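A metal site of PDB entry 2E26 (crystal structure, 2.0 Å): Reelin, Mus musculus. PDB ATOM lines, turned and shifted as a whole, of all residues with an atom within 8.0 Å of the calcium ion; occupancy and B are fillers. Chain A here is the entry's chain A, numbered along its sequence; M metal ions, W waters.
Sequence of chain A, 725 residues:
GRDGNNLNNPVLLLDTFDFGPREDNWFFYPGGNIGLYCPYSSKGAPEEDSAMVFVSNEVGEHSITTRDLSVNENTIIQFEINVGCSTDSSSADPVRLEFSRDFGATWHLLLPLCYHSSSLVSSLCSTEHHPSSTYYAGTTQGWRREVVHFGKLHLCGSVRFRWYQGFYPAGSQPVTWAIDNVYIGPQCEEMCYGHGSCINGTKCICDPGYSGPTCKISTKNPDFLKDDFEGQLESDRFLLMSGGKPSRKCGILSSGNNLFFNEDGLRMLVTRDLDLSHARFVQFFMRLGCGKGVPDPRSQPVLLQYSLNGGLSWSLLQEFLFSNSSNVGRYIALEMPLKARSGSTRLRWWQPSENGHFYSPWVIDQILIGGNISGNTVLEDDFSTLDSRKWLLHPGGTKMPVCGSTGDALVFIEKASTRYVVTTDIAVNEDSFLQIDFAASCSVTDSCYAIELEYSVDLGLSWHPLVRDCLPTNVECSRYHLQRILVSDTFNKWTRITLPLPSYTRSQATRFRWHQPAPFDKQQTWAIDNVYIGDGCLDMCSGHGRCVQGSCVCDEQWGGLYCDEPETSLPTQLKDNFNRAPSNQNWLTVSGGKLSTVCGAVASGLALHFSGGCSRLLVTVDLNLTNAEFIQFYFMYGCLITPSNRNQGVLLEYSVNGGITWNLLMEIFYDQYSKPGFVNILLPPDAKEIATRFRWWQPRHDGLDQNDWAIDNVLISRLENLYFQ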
ATOM      1  N   ASP A  15      10.200 -13.705  18.535  1.00  0.00           N
ATOM      2  CA  ASP A  15      10.099 -14.065  19.936  1.00  0.00           C
ATOM      3  C   ASP A  15       9.087 -13.196  20.679  1.00  0.00           C
ATOM      4  O   ASP A  15       9.240 -11.973  20.755  1.00  0.00           O
ATOM      5  CB  ASP A  15      11.465 -14.007  20.623  1.00  0.00           C
ATOM      6  CG  ASP A  15      11.615 -15.073  21.719  1.00  0.00           C
ATOM      7  OD1 ASP A  15      10.606 -15.427  22.365  1.00  0.00           O
ATOM      8  OD2 ASP A  15      12.752 -15.565  21.915  1.00  0.00           O
ATOM      9  N   THR A  16       8.056 -13.843  21.220  1.00  0.00           N
ATOM     10  CA  THR A  16       7.060 -13.167  22.057  1.00  0.00           C
ATOM     11  C   THR A  16       7.401 -13.364  23.539  1.00  0.00           C
ATOM     12  O   THR A  16       6.735 -12.800  24.413  1.00  0.00           O
ATOM     13  CB  THR A  16       5.644 -13.748  21.842  1.00  0.00           C
ATOM     14  OG1 THR A  16       5.657 -15.131  22.186  1.00  0.00           O
ATOM     15  CG2 THR A  16       5.173 -13.576  20.389  1.00  0.00           C
ATOM     16  N   PHE A  17       8.420 -14.196  23.813  1.00  0.00           N
ATOM     17  CA  PHE A  17       8.867 -14.509  25.188  1.00  0.00           C
ATOM     18  C   PHE A  17       7.743 -15.055  26.071  1.00  0.00           C
ATOM     19  O   PHE A  17       7.858 -15.070  27.308  1.00  0.00           O
ATOM     20  CB  PHE A  17       9.510 -13.292  25.860  1.00  0.00           C
ATOM     21  CG  PHE A  17      10.627 -12.664  25.085  1.00  0.00           C
ATOM     22  CD1 PHE A  17      10.447 -11.440  24.452  1.00  0.00           C
ATOM     23  CD2 PHE A  17      11.869 -13.288  24.985  1.00  0.00           C
ATOM     24  CE1 PHE A  17      11.498 -10.847  23.734  1.00  0.00           C
ATOM     25  CE2 PHE A  17      12.909 -12.711  24.278  1.00  0.00           C
ATOM     26  CZ  PHE A  17      12.716 -11.488  23.648  1.00  0.00           C
ATOM     27  N   ASP A  18       6.667 -15.511  25.449  1.00  0.00           N
ATOM     28  CA  ASP A  18       5.452 -15.862  26.186  1.00  0.00           C
ATOM     29  C   ASP A  18       5.541 -17.257  26.759  1.00  0.00           C
ATOM     30  O   ASP A  18       4.824 -17.606  27.699  1.00  0.00           O
ATOM     31  CB  ASP A  18       4.220 -15.665  25.316  1.00  0.00           C
ATOM     32  CG  ASP A  18       3.843 -14.202  25.182  1.00  0.00           C
ATOM     33  OD1 ASP A  18       4.345 -13.367  25.976  1.00  0.00           O
ATOM     34  OD2 ASP A  18       3.047 -13.876  24.271  1.00  0.00           O
ATOM     35  N   PHE A  19       6.444 -18.051  26.193  1.00  0.00           N
ATOM     36  CA  PHE A  19       6.865 -19.301  26.788  1.00  0.00           C
ATOM     37  C   PHE A  19       8.026 -18.933  27.714  1.00  0.00           C
ATOM     38  O   PHE A  19       7.832 -18.343  28.785  1.00  0.00           O
ATOM     39  CB  PHE A  19       7.292 -20.278  25.682  1.00  0.00           C
ATOM     40  CG  PHE A  19       6.201 -20.573  24.667  1.00  0.00           C
ATOM     41  CD1 PHE A  19       5.869 -19.644  23.682  1.00  0.00           C
ATOM     42  CD2 PHE A  19       5.512 -21.792  24.700  1.00  0.00           C
ATOM     43  CE1 PHE A  19       4.865 -19.902  22.757  1.00  0.00           C
ATOM     44  CE2 PHE A  19       4.508 -22.069  23.767  1.00  0.00           C
ATOM     45  CZ  PHE A  19       4.176 -21.121  22.790  1.00  0.00           C
ATOM     46  N   ILE A  34      13.182 -13.643  31.999  1.00  0.00           N
ATOM     47  CA  ILE A  34      11.776 -13.590  31.631  1.00  0.00           C
ATOM     48  C   ILE A  34      10.943 -13.143  32.843  1.00  0.00           C
ATOM     49  O   ILE A  34      11.124 -13.660  33.957  1.00  0.00           O
ATOM     50  CB  ILE A  34      11.271 -14.967  31.102  1.00  0.00           C
ATOM     51  CG1 ILE A  34      12.033 -15.383  29.842  1.00  0.00           C
ATOM     52  CG2 ILE A  34       9.760 -14.964  30.872  1.00  0.00           C
ATOM     53  CD1 ILE A  34      11.681 -14.616  28.578  1.00  0.00           C
ATOM     54  N   GLY A  35      10.076 -12.163  32.635  1.00  0.00           N
ATOM     55  CA  GLY A  35       9.186 -11.658  33.665  1.00  0.00           C
ATOM     56  C   GLY A  35       8.275 -10.590  33.103  1.00  0.00           C
ATOM     57  O   GLY A  35       8.194 -10.423  31.892  1.00  0.00           O
ATOM     58  N   ALA A  45      -2.743  -8.140  25.389  1.00  0.00           N
ATOM     59  CA  ALA A  45      -3.361  -9.138  26.268  1.00  0.00           C
ATOM     60  C   ALA A  45      -2.466  -9.391  27.487  1.00  0.00           C
ATOM     61  O   ALA A  45      -1.250  -9.145  27.416  1.00  0.00           O
ATOM     62  CB  ALA A  45      -3.606 -10.427  25.491  1.00  0.00           C
ATOM     63  N   PRO A  46      -3.043  -9.869  28.598  1.00  0.00           N
ATOM     64  CA  PRO A  46      -2.243 -10.080  29.796  1.00  0.00           C
ATOM     65  C   PRO A  46      -1.239 -11.221  29.600  1.00  0.00           C
ATOM     66  O   PRO A  46      -0.101 -11.114  30.048  1.00  0.00           O
ATOM     67  CB  PRO A  46      -3.280 -10.465  30.862  1.00  0.00           C
ATOM     68  CG  PRO A  46      -4.426 -11.031  30.091  1.00  0.00           C
ATOM     69  CD  PRO A  46      -4.456 -10.263  28.804  1.00  0.00           C
ATOM     70  N   GLU A  47      -1.680 -12.285  28.930  1.00  0.00           N
ATOM     71  CA  GLU A  47      -0.852 -13.460  28.636  1.00  0.00           C
ATOM     72  C   GLU A  47       0.372 -13.100  27.805  1.00  0.00           C
ATOM     73  O   GLU A  47       1.376 -13.807  27.814  1.00  0.00           O
ATOM     74  CB  GLU A  47      -1.687 -14.539  27.945  1.00  0.00           C
ATOM     75  CG  GLU A  47      -2.342 -14.121  26.627  1.00  0.00           C
ATOM     76  CD  GLU A  47      -3.551 -14.976  26.267  1.00  0.00           C
ATOM     77  OE1 GLU A  47      -3.389 -16.214  26.131  1.00  0.00           O
ATOM     78  OE2 GLU A  47      -4.661 -14.413  26.135  1.00  0.00           O
ATOM     79  N   GLU A  48       0.273 -11.982  27.091  1.00  0.00           N
ATOM     80  CA  GLU A  48       1.346 -11.498  26.249  1.00  0.00           C
ATOM     81  C   GLU A  48       2.368 -10.645  27.009  1.00  0.00           C
ATOM     82  O   GLU A  48       3.424 -10.336  26.467  1.00  0.00           O
ATOM     83  CB  GLU A  48       0.768 -10.710  25.057  1.00  0.00           C
ATOM     84  CG  GLU A  48       0.108 -11.582  23.970  1.00  0.00           C
ATOM     85  CD  GLU A  48       1.067 -11.965  22.835  1.00  0.00           C
ATOM     86  OE1 GLU A  48       1.233 -13.184  22.581  1.00  0.00           O
ATOM     87  OE2 GLU A  48       1.646 -11.057  22.188  1.00  0.00           O
ATOM     88  N   ASP A  49       2.064 -10.284  28.252  1.00  0.00           N
ATOM     89  CA  ASP A  49       2.925  -9.364  29.034  1.00  0.00           C
ATOM     90  C   ASP A  49       4.308  -9.935  29.364  1.00  0.00           C
ATOM     91  O   ASP A  49       5.245  -9.179  29.621  1.00  0.00           O
ATOM     92  CB  ASP A  49       2.230  -8.904  30.320  1.00  0.00           C
ATOM     93  CG  ASP A  49       1.180  -7.834  30.077  1.00  0.00           C
ATOM     94  OD1 ASP A  49       1.161  -7.191  29.002  1.00  0.00           O
ATOM     95  OD2 ASP A  49       0.367  -7.618  30.994  1.00  0.00           O
ATOM     96  N   SER A  50       4.419 -11.255  29.364  1.00  0.00           N
ATOM     97  CA  SER A  50       5.731 -11.899  29.561  1.00  0.00           C
ATOM     98  C   SER A  50       6.758 -11.366  28.554  1.00  0.00           C
ATOM     99  O   SER A  50       6.524 -11.350  27.339  1.00  0.00           O
ATOM    100  CB  SER A  50       5.593 -13.415  29.458  1.00  0.00           C
ATOM    101  OG  SER A  50       6.846 -14.023  29.670  1.00  0.00           O
ATOM    102  N   ALA A  51       7.888 -10.894  29.092  1.00  0.00           N
ATOM    103  CA  ALA A  51       8.903 -10.182  28.323  1.00  0.00           C
ATOM    104  C   ALA A  51      10.307 -10.489  28.850  1.00  0.00           C
ATOM    105  O   ALA A  51      10.459 -11.132  29.901  1.00  0.00           O
ATOM    106  CB  ALA A  51       8.640  -8.670  28.381  1.00  0.00           C
ATOM    107  N   MET A  52      11.336 -10.056  28.123  1.00  0.00           N
ATOM    108  CA  MET A  52      12.692 -10.190  28.602  1.00  0.00           C
ATOM    109  C   MET A  52      13.046  -8.919  29.369  1.00  0.00           C
ATOM    110  O   MET A  52      13.121  -7.835  28.786  1.00  0.00           O
ATOM    111  CB  MET A  52      13.670 -10.435  27.451  1.00  0.00           C
ATOM    112  CG  MET A  52      15.104 -10.735  27.911  1.00  0.00           C
ATOM    113  SD  MET A  52      15.263 -12.252  28.840  1.00  0.00           S
ATOM    114  CE  MET A  52      15.121 -13.471  27.531  1.00  0.00           C
ATOM    115  N   GLU A  80       8.896  -4.195  20.750  1.00  0.00           N
ATOM    116  CA  GLU A  80       8.338  -3.291  21.745  1.00  0.00           C
ATOM    117  C   GLU A  80       9.340  -3.150  22.889  1.00  0.00           C
ATOM    118  O   GLU A  80      10.048  -4.088  23.224  1.00  0.00           O
ATOM    119  CB  GLU A  80       6.993  -3.815  22.225  1.00  0.00           C
ATOM    120  CG  GLU A  80       5.942  -3.751  21.112  1.00  0.00           C
ATOM    121  CD  GLU A  80       4.855  -4.802  21.229  1.00  0.00           C
ATOM    122  OE1 GLU A  80       4.645  -5.312  22.346  1.00  0.00           O
ATOM    123  OE2 GLU A  80       4.214  -5.123  20.203  1.00  0.00           O
ATOM    124  N   TRP A 143       4.798   1.165  27.209  1.00  0.00           N
ATOM    125  CA  TRP A 143       5.529   0.408  26.204  1.00  0.00           C
ATOM    126  C   TRP A 143       5.304   1.086  24.846  1.00  0.00           C
ATOM    127  O   TRP A 143       4.292   1.751  24.632  1.00  0.00           O
ATOM    128  CB  TRP A 143       4.994  -1.013  26.151  1.00  0.00           C
ATOM    129  CG  TRP A 143       5.533  -1.910  27.242  1.00  0.00           C
ATOM    130  CD1 TRP A 143       5.104  -1.984  28.555  1.00  0.00           C
ATOM    131  CD2 TRP A 143       6.591  -2.862  27.115  1.00  0.00           C
ATOM    132  NE1 TRP A 143       5.841  -2.933  29.242  1.00  0.00           N
ATOM    133  CE2 TRP A 143       6.754  -3.487  28.375  1.00  0.00           C
ATOM    134  CE3 TRP A 143       7.406  -3.266  26.052  1.00  0.00           C
ATOM    135  CZ2 TRP A 143       7.713  -4.485  28.600  1.00  0.00           C
ATOM    136  CZ3 TRP A 143       8.349  -4.250  26.272  1.00  0.00           C
ATOM    137  CH2 TRP A 143       8.503  -4.846  27.539  1.00  0.00           C
ATOM    138  N   ILE A 179      12.289  -5.728  26.744  1.00  0.00           N
ATOM    139  CA  ILE A 179      11.806  -5.807  25.366  1.00  0.00           C
ATOM    140  C   ILE A 179      10.838  -6.952  25.200  1.00  0.00           C
ATOM    141  O   ILE A 179      10.836  -7.891  26.002  1.00  0.00           O
ATOM    142  CB  ILE A 179      12.961  -5.911  24.296  1.00  0.00           C
ATOM    143  CG1 ILE A 179      13.841  -7.155  24.512  1.00  0.00           C
ATOM    144  CG2 ILE A 179      13.802  -4.627  24.293  1.00  0.00           C
ATOM    145  CD1 ILE A 179      14.802  -7.423  23.339  1.00  0.00           C
ATOM    146  N   ASP A 180      10.004  -6.868  24.169  1.00  0.00           N
ATOM    147  CA  ASP A 180       8.997  -7.910  23.891  1.00  0.00           C
ATOM    148  C   ASP A 180       8.711  -7.947  22.396  1.00  0.00           C
ATOM    149  O   ASP A 180       9.061  -7.006  21.669  1.00  0.00           O
ATOM    150  CB  ASP A 180       7.697  -7.620  24.658  1.00  0.00           C
ATOM    151  CG  ASP A 180       6.871  -8.874  24.893  1.00  0.00           C
ATOM    152  OD1 ASP A 180       7.296  -9.964  24.473  1.00  0.00           O
ATOM    153  OD2 ASP A 180       5.797  -8.779  25.536  1.00  0.00           O
ATOM    154  N   ASN A 181       8.106  -9.038  21.936  1.00  0.00           N
ATOM    155  CA  ASN A 181       7.590  -9.141  20.563  1.00  0.00           C
ATOM    156  C   ASN A 181       8.593  -8.693  19.502  1.00  0.00           C
ATOM    157  O   ASN A 181       8.354  -7.747  18.730  1.00  0.00           O
ATOM    158  CB  ASN A 181       6.256  -8.386  20.412  1.00  0.00           C
ATOM    159  CG  ASN A 181       5.171  -8.927  21.311  1.00  0.00           C
ATOM    160  OD1 ASN A 181       4.943 -10.142  21.368  1.00  0.00           O
ATOM    161  ND2 ASN A 181       4.471  -8.022  22.002  1.00  0.00           N
ATOM    162  N   VAL A 182       9.710  -9.398  19.460  1.00  0.00           N
ATOM    163  CA  VAL A 182      10.772  -9.072  18.528  1.00  0.00           C
ATOM    164  C   VAL A 182      10.479  -9.809  17.236  1.00  0.00           C
ATOM    165  O   VAL A 182      10.202 -11.012  17.239  1.00  0.00           O
ATOM    166  CB  VAL A 182      12.156  -9.490  19.082  1.00  0.00           C
ATOM    167  CG1 VAL A 182      13.278  -9.141  18.099  1.00  0.00           C
ATOM    168  CG2 VAL A 182      12.405  -8.835  20.436  1.00  0.00           C
HETATM  169 CA    CA M   1       5.385 -11.232  25.424  1.00  0.00          CA
HETATM  170  O   HOH W   1       4.210 -11.089  23.703  1.00  0.00           O
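O of Phe 17 lies within hydrogen-bond range of OG of Ser 50, 2.8 Å away. N of Asp 180 lies within hydrogen-bond range of O of Glu 80, 2.9 Å away.
The nearest printed residue that does not touch the calcium ion is Asn 181 (4.2 Å).
Water W1 is bound to the calcium ion (2.1 Å). The backbone carbonyl oxygen (O) of Ser 50 is bound to the calcium ion. O of Thr 16 binds the calcium ion, 2.3 Å away. The backbone carbonyl oxygen (O) of Glu 48 is bound to the calcium ion (2.4 Å). The calcium ion is bound by OD1 of Asp 18 (2.4 Å). The calcium ion is bound by OD1 of Asp 180, at 2.5 Å. The calcium ion is bound by the side-chain carboxylate (OD2) of Asp 180 (2.5 Å). The calcium ion has seven donor atoms within binding distance.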
